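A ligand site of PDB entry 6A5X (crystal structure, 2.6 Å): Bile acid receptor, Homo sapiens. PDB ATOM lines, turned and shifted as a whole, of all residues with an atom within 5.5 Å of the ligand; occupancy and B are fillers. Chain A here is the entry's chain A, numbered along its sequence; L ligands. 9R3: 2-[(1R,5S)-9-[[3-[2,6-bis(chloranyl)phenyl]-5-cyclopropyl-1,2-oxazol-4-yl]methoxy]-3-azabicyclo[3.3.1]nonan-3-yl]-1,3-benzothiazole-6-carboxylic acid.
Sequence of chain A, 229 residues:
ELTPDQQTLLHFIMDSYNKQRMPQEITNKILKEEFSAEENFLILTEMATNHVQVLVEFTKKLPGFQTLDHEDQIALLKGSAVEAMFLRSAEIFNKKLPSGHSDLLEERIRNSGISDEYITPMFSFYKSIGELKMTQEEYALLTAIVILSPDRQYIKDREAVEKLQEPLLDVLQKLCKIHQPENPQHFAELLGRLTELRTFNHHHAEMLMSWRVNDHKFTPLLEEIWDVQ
The guanidinium group (NH1) of Arg 88 lies within salt-bridge range of an oxygen (O4) of the ligand (3.0 Å). An oxygen (O3) of the ligand lies within hydrogen-bond range of the side-chain hydroxyl of Ser 99.
O of Ile 92 is in hydrogen-bond range of N of Leu 97. The backbone carbonyl oxygen (O) of Phe 41 is in hydrogen-bond range of the side-chain hydroxyl (OG1) of Thr 45, 3.1 Å away. O of Phe 86 lies within hydrogen-bond range of OG of Ser 89. SD of Met 22 lies within hydrogen-bond range of N of His 51 (3.5 Å). OG of Ser 89 lies within hydrogen-bond range of OH of Tyr 126 (2.8 Å).
Arg 21 touches the ligand. Met 22 touches the ligand (N to O4, 3.9 Å). Thr 27 touches the ligand (CG2 to C26, 3.6 Å). Ile 30 touches the ligand (CD1 to C25, 3.99 Å). Phe 41 touches the ligand (CE2 to C8, 3.8 Å). O of Leu 44 touches C4 of the ligand, 3.7 Å away. Thr 45 touches the ligand (OG1 to C8, 3.4 Å). Met 47 touches the ligand. Ala 48 touches the ligand (CB to O2, 3.9 Å). His 51 touches the ligand (CB to C18, 3.8 Å). O of Met 85 touches C20 of the ligand, at 3.5 Å. CD1 of Phe 86 touches C10 of the ligand (3.3 Å). Ser 89 touches the ligand (CB to C22, 3.6 Å). CD1 of Ile 92 touches C23 of the ligand, 3.4 Å away. Gly 100 touches the ligand (CA to C25, 3.7 Å). CD1 of Ile 114 touches CL1 of the ligand (3.98 Å). Met 122 touches the ligand. OH of Tyr 126 touches C11 of the ligand (3.5 Å). His 204 touches the ligand. CZ3 of Trp 211 touches O1 of the ligand (3.4 Å). Phe 218 touches the ligand (CD1 to C7, 3.8 Å). Trp 226 touches the ligand. 24 residues have an atom within 4 Å of the ligand: Arg 21, Met 22, Thr 27, Ile 30, Phe 41, Leu 44, Thr 45, Met 47, Ala 48, His 51, Met 85, Phe 86, Arg 88, Ser 89, Ile 92, Ser 99, Gly 100, Ile 114, Met 122, Tyr 126, His 204, Trp 211, Phe 218 and Trp 226.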
ATOM      1  N   GLN A  20     -11.269  20.150 -15.915  1.00  0.00           N
ATOM      2  CA  GLN A  20     -10.874  20.224 -14.516  1.00  0.00           C
ATOM      3  C   GLN A  20     -11.708  19.346 -13.567  1.00  0.00           C
ATOM      4  O   GLN A  20     -11.558  19.457 -12.343  1.00  0.00           O
ATOM      5  CB  GLN A  20     -10.844  21.713 -14.062  1.00  0.00           C
ATOM      6  CG  GLN A  20     -12.052  22.231 -13.263  1.00  0.00           C
ATOM      7  CD  GLN A  20     -11.778  23.496 -12.482  1.00  0.00           C
ATOM      8  OE1 GLN A  20     -12.608  23.886 -11.644  1.00  0.00           O
ATOM      9  NE2 GLN A  20     -10.632  24.155 -12.725  1.00  0.00           N
ATOM     10  N   ARG A  21     -12.574  18.478 -14.080  1.00  0.00           N
ATOM     11  CA  ARG A  21     -13.479  17.743 -13.202  1.00  0.00           C
ATOM     12  C   ARG A  21     -12.772  16.770 -12.251  1.00  0.00           C
ATOM     13  O   ARG A  21     -11.735  16.168 -12.577  1.00  0.00           O
ATOM     14  CB  ARG A  21     -14.590  17.025 -13.992  1.00  0.00           C
ATOM     15  CG  ARG A  21     -15.604  17.968 -14.622  1.00  0.00           C
ATOM     16  CD  ARG A  21     -16.516  18.594 -13.571  1.00  0.00           C
ATOM     17  NE  ARG A  21     -17.399  19.638 -14.090  1.00  0.00           N
ATOM     18  CZ  ARG A  21     -17.040  20.889 -14.422  1.00  0.00           C
ATOM     19  NH1 ARG A  21     -15.774  21.301 -14.347  1.00  0.00           N
ATOM     20  NH2 ARG A  21     -17.977  21.728 -14.861  1.00  0.00           N
ATOM     21  N   MET A  22     -13.339  16.666 -11.052  1.00  0.00           N
ATOM     22  CA  MET A  22     -12.861  15.781 -10.022  1.00  0.00           C
ATOM     23  C   MET A  22     -13.700  14.549 -10.094  1.00  0.00           C
ATOM     24  O   MET A  22     -14.898  14.618 -10.348  1.00  0.00           O
ATOM     25  CB  MET A  22     -13.054  16.380  -8.656  1.00  0.00           C
ATOM     26  CG  MET A  22     -12.623  17.814  -8.513  1.00  0.00           C
ATOM     27  SD  MET A  22     -11.780  18.050  -6.956  1.00  0.00           S
ATOM     28  CE  MET A  22     -12.930  17.404  -5.754  1.00  0.00           C
ATOM     29  N   THR A  27     -16.321  12.939  -5.194  1.00  0.00           N
ATOM     30  CA  THR A  27     -17.337  13.907  -4.871  1.00  0.00           C
ATOM     31  C   THR A  27     -18.607  13.250  -4.342  1.00  0.00           C
ATOM     32  O   THR A  27     -19.370  13.909  -3.610  1.00  0.00           O
ATOM     33  CB  THR A  27     -17.641  14.859  -6.027  1.00  0.00           C
ATOM     34  OG1 THR A  27     -17.964  14.112  -7.207  1.00  0.00           O
ATOM     35  CG2 THR A  27     -16.433  15.719  -6.281  1.00  0.00           C
ATOM     36  N   ILE A  30     -19.458  13.612  -0.590  1.00  0.00           N
ATOM     37  CA  ILE A  30     -20.256  14.703  -0.060  1.00  0.00           C
ATOM     38  C   ILE A  30     -21.655  14.192   0.380  1.00  0.00           C
ATOM     39  O   ILE A  30     -22.140  14.500   1.467  1.00  0.00           O
ATOM     40  CB  ILE A  30     -20.340  15.930  -1.015  1.00  0.00           C
ATOM     41  CG1 ILE A  30     -18.977  16.608  -1.173  1.00  0.00           C
ATOM     42  CG2 ILE A  30     -21.286  16.984  -0.462  1.00  0.00           C
ATOM     43  CD1 ILE A  30     -18.838  17.427  -2.463  1.00  0.00           C
ATOM     44  N   PHE A  41     -15.520  17.976   8.280  1.00  0.00           N
ATOM     45  CA  PHE A  41     -14.180  18.545   8.070  1.00  0.00           C
ATOM     46  C   PHE A  41     -13.296  17.644   7.227  1.00  0.00           C
ATOM     47  O   PHE A  41     -12.658  18.099   6.321  1.00  0.00           O
ATOM     48  CB  PHE A  41     -13.502  18.860   9.406  1.00  0.00           C
ATOM     49  CG  PHE A  41     -12.097  19.351   9.267  1.00  0.00           C
ATOM     50  CD1 PHE A  41     -11.031  18.448   9.193  1.00  0.00           C
ATOM     51  CD2 PHE A  41     -11.821  20.706   9.153  1.00  0.00           C
ATOM     52  CE1 PHE A  41      -9.738  18.890   9.028  1.00  0.00           C
ATOM     53  CE2 PHE A  41     -10.512  21.143   9.002  1.00  0.00           C
ATOM     54  CZ  PHE A  41      -9.477  20.239   8.928  1.00  0.00           C
ATOM     55  N   LEU A  44     -14.394  18.031   3.625  1.00  0.00           N
ATOM     56  CA  LEU A  44     -14.001  19.326   3.073  1.00  0.00           C
ATOM     57  C   LEU A  44     -12.504  19.343   2.753  1.00  0.00           C
ATOM     58  O   LEU A  44     -12.089  19.806   1.691  1.00  0.00           O
ATOM     59  CB  LEU A  44     -14.377  20.452   4.030  1.00  0.00           C
ATOM     60  CG  LEU A  44     -15.869  20.672   4.266  1.00  0.00           C
ATOM     61  CD1 LEU A  44     -16.072  21.849   5.193  1.00  0.00           C
ATOM     62  CD2 LEU A  44     -16.669  20.869   2.980  1.00  0.00           C
ATOM     63  N   THR A  45     -11.698  18.785   3.669  1.00  0.00           N
ATOM     64  CA  THR A  45     -10.249  18.630   3.455  1.00  0.00           C
ATOM     65  C   THR A  45      -9.876  17.826   2.195  1.00  0.00           C
ATOM     66  O   THR A  45      -8.963  18.164   1.454  1.00  0.00           O
ATOM     67  CB  THR A  45      -9.594  18.076   4.704  1.00  0.00           C
ATOM     68  OG1 THR A  45      -9.777  19.017   5.769  1.00  0.00           O
ATOM     69  CG2 THR A  45      -8.145  17.840   4.503  1.00  0.00           C
ATOM     70  N   MET A  47     -11.978  17.261  -0.504  1.00  0.00           N
ATOM     71  CA  MET A  47     -12.427  17.945  -1.706  1.00  0.00           C
ATOM     72  C   MET A  47     -11.448  19.030  -2.042  1.00  0.00           C
ATOM     73  O   MET A  47     -11.117  19.257  -3.196  1.00  0.00           O
ATOM     74  CB  MET A  47     -13.817  18.556  -1.525  1.00  0.00           C
ATOM     75  CG  MET A  47     -14.976  17.591  -1.353  1.00  0.00           C
ATOM     76  SD  MET A  47     -14.986  16.166  -2.467  1.00  0.00           S
ATOM     77  CE  MET A  47     -14.489  14.832  -1.385  1.00  0.00           C
ATOM     78  N   ALA A  48     -10.946  19.694  -1.014  1.00  0.00           N
ATOM     79  CA  ALA A  48      -9.972  20.784  -1.168  1.00  0.00           C
ATOM     80  C   ALA A  48      -8.617  20.305  -1.694  1.00  0.00           C
ATOM     81  O   ALA A  48      -8.085  20.953  -2.582  1.00  0.00           O
ATOM     82  CB  ALA A  48      -9.783  21.501   0.156  1.00  0.00           C
ATOM     83  N   HIS A  51      -9.120  19.464  -5.135  1.00  0.00           N
ATOM     84  CA  HIS A  51      -9.406  20.624  -5.940  1.00  0.00           C
ATOM     85  C   HIS A  51      -8.133  21.393  -6.286  1.00  0.00           C
ATOM     86  O   HIS A  51      -7.993  21.799  -7.425  1.00  0.00           O
ATOM     87  CB  HIS A  51     -10.402  21.554  -5.295  1.00  0.00           C
ATOM     88  CG  HIS A  51     -10.751  22.725  -6.163  1.00  0.00           C
ATOM     89  ND1 HIS A  51     -11.266  22.578  -7.441  1.00  0.00           N
ATOM     90  CD2 HIS A  51     -10.598  24.052  -5.969  1.00  0.00           C
ATOM     91  CE1 HIS A  51     -11.445  23.767  -7.980  1.00  0.00           C
ATOM     92  NE2 HIS A  51     -11.052  24.679  -7.106  1.00  0.00           N
ATOM     93  N   VAL A  82      -7.133  30.562  -2.334  1.00  0.00           N
ATOM     94  CA  VAL A  82      -8.389  30.799  -1.620  1.00  0.00           C
ATOM     95  C   VAL A  82      -9.467  31.425  -2.492  1.00  0.00           C
ATOM     96  O   VAL A  82     -10.587  30.927  -2.549  1.00  0.00           O
ATOM     97  CB  VAL A  82      -8.173  31.666  -0.374  1.00  0.00           C
ATOM     98  CG1 VAL A  82      -9.482  32.074   0.254  1.00  0.00           C
ATOM     99  CG2 VAL A  82      -7.352  30.920   0.642  1.00  0.00           C
ATOM    100  N   MET A  85     -10.727  29.059  -4.969  1.00  0.00           N
ATOM    101  CA  MET A  85     -11.523  28.008  -4.315  1.00  0.00           C
ATOM    102  C   MET A  85     -12.898  28.514  -3.944  1.00  0.00           C
ATOM    103  O   MET A  85     -13.901  27.812  -4.155  1.00  0.00           O
ATOM    104  CB  MET A  85     -10.780  27.423  -3.114  1.00  0.00           C
ATOM    105  CG  MET A  85      -9.539  26.640  -3.532  1.00  0.00           C
ATOM    106  SD  MET A  85      -8.403  26.019  -2.251  1.00  0.00           S
ATOM    107  CE  MET A  85      -9.386  24.659  -1.652  1.00  0.00           C
ATOM    108  N   PHE A  86     -12.973  29.750  -3.460  1.00  0.00           N
ATOM    109  CA  PHE A  86     -14.285  30.361  -3.160  1.00  0.00           C
ATOM    110  C   PHE A  86     -15.153  30.569  -4.398  1.00  0.00           C
ATOM    111  O   PHE A  86     -16.363  30.479  -4.300  1.00  0.00           O
ATOM    112  CB  PHE A  86     -14.139  31.695  -2.488  1.00  0.00           C
ATOM    113  CG  PHE A  86     -14.170  31.645  -1.008  1.00  0.00           C
ATOM    114  CD1 PHE A  86     -13.006  31.378  -0.278  1.00  0.00           C
ATOM    115  CD2 PHE A  86     -15.357  31.882  -0.315  1.00  0.00           C
ATOM    116  CE1 PHE A  86     -13.018  31.340   1.145  1.00  0.00           C
ATOM    117  CE2 PHE A  86     -15.384  31.830   1.087  1.00  0.00           C
ATOM    118  CZ  PHE A  86     -14.210  31.572   1.824  1.00  0.00           C
ATOM    119  N   ARG A  88     -15.042  28.627  -7.122  1.00  0.00           N
ATOM    120  CA  ARG A  88     -15.502  27.298  -7.540  1.00  0.00           C
ATOM    121  C   ARG A  88     -16.746  26.850  -6.746  1.00  0.00           C
ATOM    122  O   ARG A  88     -17.717  26.379  -7.353  1.00  0.00           O
ATOM    123  CB  ARG A  88     -14.401  26.253  -7.465  1.00  0.00           C
ATOM    124  CG  ARG A  88     -14.421  25.401  -8.726  1.00  0.00           C
ATOM    125  CD  ARG A  88     -15.496  24.344  -8.641  1.00  0.00           C
ATOM    126  NE  ARG A  88     -16.343  24.323  -9.840  1.00  0.00           N
ATOM    127  CZ  ARG A  88     -16.376  23.360 -10.764  1.00  0.00           C
ATOM    128  NH1 ARG A  88     -15.581  22.293 -10.694  1.00  0.00           N
ATOM    129  NH2 ARG A  88     -17.218  23.482 -11.778  1.00  0.00           N
ATOM    130  N   SER A  89     -16.728  27.054  -5.418  1.00  0.00           N
ATOM    131  CA  SER A  89     -17.851  26.743  -4.605  1.00  0.00           C
ATOM    132  C   SER A  89     -19.052  27.653  -4.895  1.00  0.00           C
ATOM    133  O   SER A  89     -20.207  27.205  -4.865  1.00  0.00           O
ATOM    134  CB  SER A  89     -17.483  26.837  -3.150  1.00  0.00           C
ATOM    135  OG  SER A  89     -17.134  28.129  -2.788  1.00  0.00           O
ATOM    136  N   ILE A  92     -20.705  26.110  -7.737  1.00  0.00           N
ATOM    137  CA  ILE A  92     -21.466  24.944  -7.253  1.00  0.00           C
ATOM    138  C   ILE A  92     -22.815  25.333  -6.636  1.00  0.00           C
ATOM    139  O   ILE A  92     -23.844  24.833  -7.037  1.00  0.00           O
ATOM    140  CB  ILE A  92     -20.654  24.100  -6.235  1.00  0.00           C
ATOM    141  CG1 ILE A  92     -19.494  23.412  -6.961  1.00  0.00           C
ATOM    142  CG2 ILE A  92     -21.539  23.057  -5.530  1.00  0.00           C
ATOM    143  CD1 ILE A  92     -18.410  22.938  -6.037  1.00  0.00           C
ATOM    144  N   LEU A  97     -24.488  22.372  -9.422  1.00  0.00           N
ATOM    145  CA  LEU A  97     -23.838  21.253 -10.118  1.00  0.00           C
ATOM    146  C   LEU A  97     -24.227  19.964  -9.415  1.00  0.00           C
ATOM    147  O   LEU A  97     -24.014  19.850  -8.214  1.00  0.00           O
ATOM    148  CB  LEU A  97     -22.312  21.330 -10.120  1.00  0.00           C
ATOM    149  CG  LEU A  97     -21.647  22.063 -11.268  1.00  0.00           C
ATOM    150  CD1 LEU A  97     -21.880  23.580 -11.136  1.00  0.00           C
ATOM    151  CD2 LEU A  97     -20.158  21.688 -11.272  1.00  0.00           C
ATOM    152  N   SER A  99     -22.869  17.057  -9.274  1.00  0.00           N
ATOM    153  CA  SER A  99     -21.738  16.435  -8.598  1.00  0.00           C
ATOM    154  C   SER A  99     -21.156  17.258  -7.419  1.00  0.00           C
ATOM    155  O   SER A  99     -20.338  16.758  -6.624  1.00  0.00           O
ATOM    156  CB  SER A  99     -20.671  16.128  -9.624  1.00  0.00           C
ATOM    157  OG  SER A  99     -20.317  17.313 -10.313  1.00  0.00           O
ATOM    158  N   GLY A 100     -21.540  18.521  -7.342  1.00  0.00           N
ATOM    159  CA  GLY A 100     -21.252  19.294  -6.176  1.00  0.00           C
ATOM    160  C   GLY A 100     -22.158  19.027  -4.983  1.00  0.00           C
ATOM    161  O   GLY A 100     -21.763  19.303  -3.855  1.00  0.00           O
ATOM    162  N   LEU A 105     -23.377  19.814   0.729  1.00  0.00           N
ATOM    163  CA  LEU A 105     -22.115  20.536   0.860  1.00  0.00           C
ATOM    164  C   LEU A 105     -22.312  21.696   1.860  1.00  0.00           C
ATOM    165  O   LEU A 105     -21.521  21.875   2.784  1.00  0.00           O
ATOM    166  CB  LEU A 105     -21.611  21.002  -0.476  1.00  0.00           C
ATOM    167  CG  LEU A 105     -20.202  21.590  -0.507  1.00  0.00           C
ATOM    168  CD1 LEU A 105     -19.203  20.535  -0.086  1.00  0.00           C
ATOM    169  CD2 LEU A 105     -19.821  22.145  -1.862  1.00  0.00           C
ATOM    170  N   ILE A 109     -20.303  22.350   5.425  1.00  0.00           N
ATOM    171  CA  ILE A 109     -19.580  23.568   5.687  1.00  0.00           C
ATOM    172  C   ILE A 109     -20.102  24.177   6.963  1.00  0.00           C
ATOM    173  O   ILE A 109     -19.327  24.723   7.769  1.00  0.00           O
ATOM    174  CB  ILE A 109     -19.684  24.578   4.513  1.00  0.00           C
ATOM    175  CG1 ILE A 109     -18.942  24.044   3.290  1.00  0.00           C
ATOM    176  CG2 ILE A 109     -19.121  25.962   4.854  1.00  0.00           C
ATOM    177  CD1 ILE A 109     -19.124  24.892   2.056  1.00  0.00           C
ATOM    178  N   ILE A 114     -16.303  26.023  11.719  1.00  0.00           N
ATOM    179  CA  ILE A 114     -16.095  27.389  11.266  1.00  0.00           C
ATOM    180  C   ILE A 114     -17.012  28.340  12.061  1.00  0.00           C
ATOM    181  O   ILE A 114     -18.198  28.091  12.240  1.00  0.00           O
ATOM    182  CB  ILE A 114     -16.429  27.549   9.768  1.00  0.00           C
ATOM    183  CG1 ILE A 114     -15.661  26.553   8.936  1.00  0.00           C
ATOM    184  CG2 ILE A 114     -16.070  28.956   9.283  1.00  0.00           C
ATOM    185  CD1 ILE A 114     -16.169  26.440   7.514  1.00  0.00           C
ATOM    186  N   MET A 122     -19.773  34.399   4.156  1.00  0.00           N
ATOM    187  CA  MET A 122     -19.503  33.404   3.100  1.00  0.00           C
ATOM    188  C   MET A 122     -20.744  33.145   2.277  1.00  0.00           C
ATOM    189  O   MET A 122     -20.678  33.177   1.041  1.00  0.00           O
ATOM    190  CB  MET A 122     -18.973  32.126   3.739  1.00  0.00           C
ATOM    191  CG  MET A 122     -18.675  30.954   2.781  1.00  0.00           C
ATOM    192  SD  MET A 122     -18.088  29.472   3.677  1.00  0.00           S
ATOM    193  CE  MET A 122     -17.019  30.224   4.898  1.00  0.00           C
ATOM    194  N   TYR A 126     -22.037  34.063  -1.690  1.00  0.00           N
ATOM    195  CA  TYR A 126     -22.577  33.102  -2.647  1.00  0.00           C
ATOM    196  C   TYR A 126     -23.892  33.539  -3.226  1.00  0.00           C
ATOM    197  O   TYR A 126     -24.126  33.376  -4.433  1.00  0.00           O
ATOM    198  CB  TYR A 126     -22.760  31.703  -2.051  1.00  0.00           C
ATOM    199  CG  TYR A 126     -21.511  30.980  -1.601  1.00  0.00           C
ATOM    200  CD1 TYR A 126     -20.368  30.990  -2.358  1.00  0.00           C
ATOM    201  CD2 TYR A 126     -21.489  30.285  -0.419  1.00  0.00           C
ATOM    202  CE1 TYR A 126     -19.250  30.301  -1.951  1.00  0.00           C
ATOM    203  CE2 TYR A 126     -20.359  29.605   0.018  1.00  0.00           C
ATOM    204  CZ  TYR A 126     -19.243  29.609  -0.751  1.00  0.00           C
ATOM    205  OH  TYR A 126     -18.132  28.932  -0.354  1.00  0.00           O
ATOM    206  N   HIS A 204     -10.011  33.370   5.920  1.00  0.00           N
ATOM    207  CA  HIS A 204      -9.559  32.021   5.740  1.00  0.00           C
ATOM    208  C   HIS A 204      -8.336  31.735   6.609  1.00  0.00           C
ATOM    209  O   HIS A 204      -8.165  30.629   7.098  1.00  0.00           O
ATOM    210  CB  HIS A 204      -9.288  31.732   4.277  1.00  0.00           C
ATOM    211  CG  HIS A 204      -8.945  30.310   3.995  1.00  0.00           C
ATOM    212  ND1 HIS A 204      -9.897  29.339   3.819  1.00  0.00           N
ATOM    213  CD2 HIS A 204      -7.734  29.699   3.876  1.00  0.00           C
ATOM    214  CE1 HIS A 204      -9.293  28.180   3.578  1.00  0.00           C
ATOM    215  NE2 HIS A 204      -7.993  28.361   3.617  1.00  0.00           N
ATOM    216  N   MET A 207      -9.687  31.152  10.003  1.00  0.00           N
ATOM    217  CA  MET A 207     -10.343  29.839   9.965  1.00  0.00           C
ATOM    218  C   MET A 207      -9.291  28.719  10.173  1.00  0.00           C
ATOM    219  O   MET A 207      -9.526  27.749  10.845  1.00  0.00           O
ATOM    220  CB  MET A 207     -11.051  29.635   8.617  1.00  0.00           C
ATOM    221  CG  MET A 207     -12.470  30.202   8.520  1.00  0.00           C
ATOM    222  SD  MET A 207     -13.153  30.476   6.829  1.00  0.00           S
ATOM    223  CE  MET A 207     -13.265  28.807   6.193  1.00  0.00           C
ATOM    224  N   LEU A 208      -8.145  28.864   9.540  1.00  0.00           N
ATOM    225  CA  LEU A 208      -7.121  27.874   9.575  1.00  0.00           C
ATOM    226  C   LEU A 208      -6.531  27.743  10.972  1.00  0.00           C
ATOM    227  O   LEU A 208      -6.345  26.640  11.480  1.00  0.00           O
ATOM    228  CB  LEU A 208      -6.035  28.227   8.595  1.00  0.00           C
ATOM    229  CG  LEU A 208      -6.353  28.045   7.123  1.00  0.00           C
ATOM    230  CD1 LEU A 208      -5.053  28.032   6.333  1.00  0.00           C
ATOM    231  CD2 LEU A 208      -7.155  26.770   6.832  1.00  0.00           C
ATOM    232  N   TRP A 211      -9.132  26.030  13.348  1.00  0.00           N
ATOM    233  CA  TRP A 211      -8.974  24.608  13.046  1.00  0.00           C
ATOM    234  C   TRP A 211      -7.734  23.987  13.649  1.00  0.00           C
ATOM    235  O   TRP A 211      -7.826  22.932  14.280  1.00  0.00           O
ATOM    236  CB  TRP A 211      -8.988  24.359  11.531  1.00  0.00           C
ATOM    237  CG  TRP A 211     -10.373  24.211  10.986  1.00  0.00           C
ATOM    238  CD1 TRP A 211     -11.411  23.638  11.599  1.00  0.00           C
ATOM    239  CD2 TRP A 211     -10.860  24.655   9.707  1.00  0.00           C
ATOM    240  NE1 TRP A 211     -12.528  23.678  10.794  1.00  0.00           N
ATOM    241  CE2 TRP A 211     -12.211  24.278   9.616  1.00  0.00           C
ATOM    242  CE3 TRP A 211     -10.285  25.335   8.631  1.00  0.00           C
ATOM    243  CZ2 TRP A 211     -13.005  24.570   8.529  1.00  0.00           C
ATOM    244  CZ3 TRP A 211     -11.068  25.608   7.540  1.00  0.00           C
ATOM    245  CH2 TRP A 211     -12.424  25.234   7.494  1.00  0.00           C
ATOM    246  N   PHE A 218      -4.343  19.405   7.942  1.00  0.00           N
ATOM    247  CA  PHE A 218      -4.676  19.411   6.563  1.00  0.00           C
ATOM    248  C   PHE A 218      -3.771  18.414   5.859  1.00  0.00           C
ATOM    249  O   PHE A 218      -3.135  17.596   6.484  1.00  0.00           O
ATOM    250  CB  PHE A 218      -4.521  20.875   6.074  1.00  0.00           C
ATOM    251  CG  PHE A 218      -5.203  21.853   6.964  1.00  0.00           C
ATOM    252  CD1 PHE A 218      -6.599  21.931   6.995  1.00  0.00           C
ATOM    253  CD2 PHE A 218      -4.498  22.645   7.821  1.00  0.00           C
ATOM    254  CE1 PHE A 218      -7.248  22.804   7.854  1.00  0.00           C
ATOM    255  CE2 PHE A 218      -5.157  23.528   8.681  1.00  0.00           C
ATOM    256  CZ  PHE A 218      -6.527  23.602   8.697  1.00  0.00           C
ATOM    257  N   LEU A 222      -2.148  21.120   0.874  1.00  0.00           N
ATOM    258  CA  LEU A 222      -2.858  22.288   1.410  1.00  0.00           C
ATOM    259  C   LEU A 222      -1.943  23.065   2.302  1.00  0.00           C
ATOM    260  O   LEU A 222      -1.986  24.270   2.320  1.00  0.00           O
ATOM    261  CB  LEU A 222      -4.083  21.859   2.184  1.00  0.00           C
ATOM    262  CG  LEU A 222      -5.226  21.221   1.381  1.00  0.00           C
ATOM    263  CD1 LEU A 222      -6.316  20.757   2.314  1.00  0.00           C
ATOM    264  CD2 LEU A 222      -5.813  22.136   0.370  1.00  0.00           C
ATOM    265  N   TRP A 226      -1.473  26.870   1.213  1.00  0.00           N
ATOM    266  CA  TRP A 226      -2.019  27.787   2.218  1.00  0.00           C
ATOM    267  C   TRP A 226      -1.006  28.268   3.219  1.00  0.00           C
ATOM    268  O   TRP A 226      -1.346  28.964   4.152  1.00  0.00           O
ATOM    269  CB  TRP A 226      -3.186  27.148   2.986  1.00  0.00           C
ATOM    270  CG  TRP A 226      -4.419  27.006   2.168  1.00  0.00           C
ATOM    271  CD1 TRP A 226      -4.762  27.702   1.030  1.00  0.00           C
ATOM    272  CD2 TRP A 226      -5.534  26.166   2.463  1.00  0.00           C
ATOM    273  NE1 TRP A 226      -6.010  27.316   0.586  1.00  0.00           N
ATOM    274  CE2 TRP A 226      -6.509  26.375   1.459  1.00  0.00           C
ATOM    275  CE3 TRP A 226      -5.805  25.252   3.485  1.00  0.00           C
ATOM    276  CZ2 TRP A 226      -7.730  25.696   1.440  1.00  0.00           C
ATOM    277  CZ3 TRP A 226      -7.029  24.551   3.468  1.00  0.00           C
ATOM    278  CH2 TRP A 226      -7.980  24.803   2.467  1.00  0.00           C
HETATM  279  O4  9R3 L   1     -16.074  19.340 -10.224  1.00  0.00           O
HETATM  280  C29 9R3 L   1     -16.871  18.921  -9.372  1.00  0.00           C
HETATM  281  O3  9R3 L   1     -17.800  18.149  -9.698  1.00  0.00           O
HETATM  282  C27 9R3 L   1     -16.721  19.387  -7.959  1.00  0.00           C
HETATM  283  C26 9R3 L   1     -17.689  19.014  -7.024  1.00  0.00           C
HETATM  284  C25 9R3 L   1     -17.631  19.425  -5.700  1.00  0.00           C
HETATM  285  C23 9R3 L   1     -16.574  20.199  -5.282  1.00  0.00           C
HETATM  286  N3  9R3 L   1     -16.345  20.743  -4.059  1.00  0.00           N
HETATM  287  C28 9R3 L   1     -15.650  20.195  -7.544  1.00  0.00           C
HETATM  288  C24 9R3 L   1     -15.600  20.577  -6.201  1.00  0.00           C
HETATM  289  S1  9R3 L   1     -14.395  21.532  -5.542  1.00  0.00           S
HETATM  290  C21 9R3 L   1     -15.192  21.465  -4.047  1.00  0.00           C
HETATM  291  N2  9R3 L   1     -14.668  22.027  -2.950  1.00  0.00           N
HETATM  292  C16 9R3 L   1     -15.504  22.015  -1.743  1.00  0.00           C
HETATM  293  C18 9R3 L   1     -13.279  22.469  -3.024  1.00  0.00           C
HETATM  294  C17 9R3 L   1     -13.046  23.542  -1.972  1.00  0.00           C
HETATM  295  C20 9R3 L   1     -13.802  24.795  -2.407  1.00  0.00           C
HETATM  296  C22 9R3 L   1     -14.696  25.358  -1.329  1.00  0.00           C
HETATM  297  C19 9R3 L   1     -15.683  24.335  -0.824  1.00  0.00           C
HETATM  298  C14 9R3 L   1     -14.994  22.951  -0.670  1.00  0.00           C
HETATM  299  C15 9R3 L   1     -13.470  22.985  -0.644  1.00  0.00           C
HETATM  300  O2  9R3 L   1     -12.882  23.804   0.352  1.00  0.00           O
HETATM  301  C6  9R3 L   1     -13.216  23.436   1.675  1.00  0.00           C
HETATM  302  C2  9R3 L   1     -12.373  24.260   2.605  1.00  0.00           C
HETATM  303  C1  9R3 L   1     -11.397  23.787   3.571  1.00  0.00           C
HETATM  304  C4  9R3 L   1     -10.866  22.464   3.966  1.00  0.00           C
HETATM  305  C8  9R3 L   1     -11.146  22.150   5.432  1.00  0.00           C
HETATM  306  C7  9R3 L   1      -9.729  22.423   4.970  1.00  0.00           C
HETATM  307  O1  9R3 L   1     -10.959  24.875   4.191  1.00  0.00           O
HETATM  308  C3  9R3 L   1     -12.361  25.727   2.783  1.00  0.00           C
HETATM  309  N1  9R3 L   1     -11.487  26.015   3.769  1.00  0.00           N
HETATM  310  C5  9R3 L   1     -13.215  26.668   1.982  1.00  0.00           C
HETATM  311  C13 9R3 L   1     -14.569  26.801   2.289  1.00  0.00           C
HETATM  312 CL1  9R3 L   1     -15.206  25.894   3.695  1.00  0.00          CL
HETATM  313  C12 9R3 L   1     -15.363  27.658   1.544  1.00  0.00           C
HETATM  314  C11 9R3 L   1     -14.788  28.329   0.464  1.00  0.00           C
HETATM  315  C10 9R3 L   1     -13.443  28.186   0.150  1.00  0.00           C
HETATM  316  C9  9R3 L   1     -12.663  27.383   0.923  1.00  0.00           C
HETATM  317 CL2  9R3 L   1     -10.938  27.181   0.527  1.00  0.00          CL
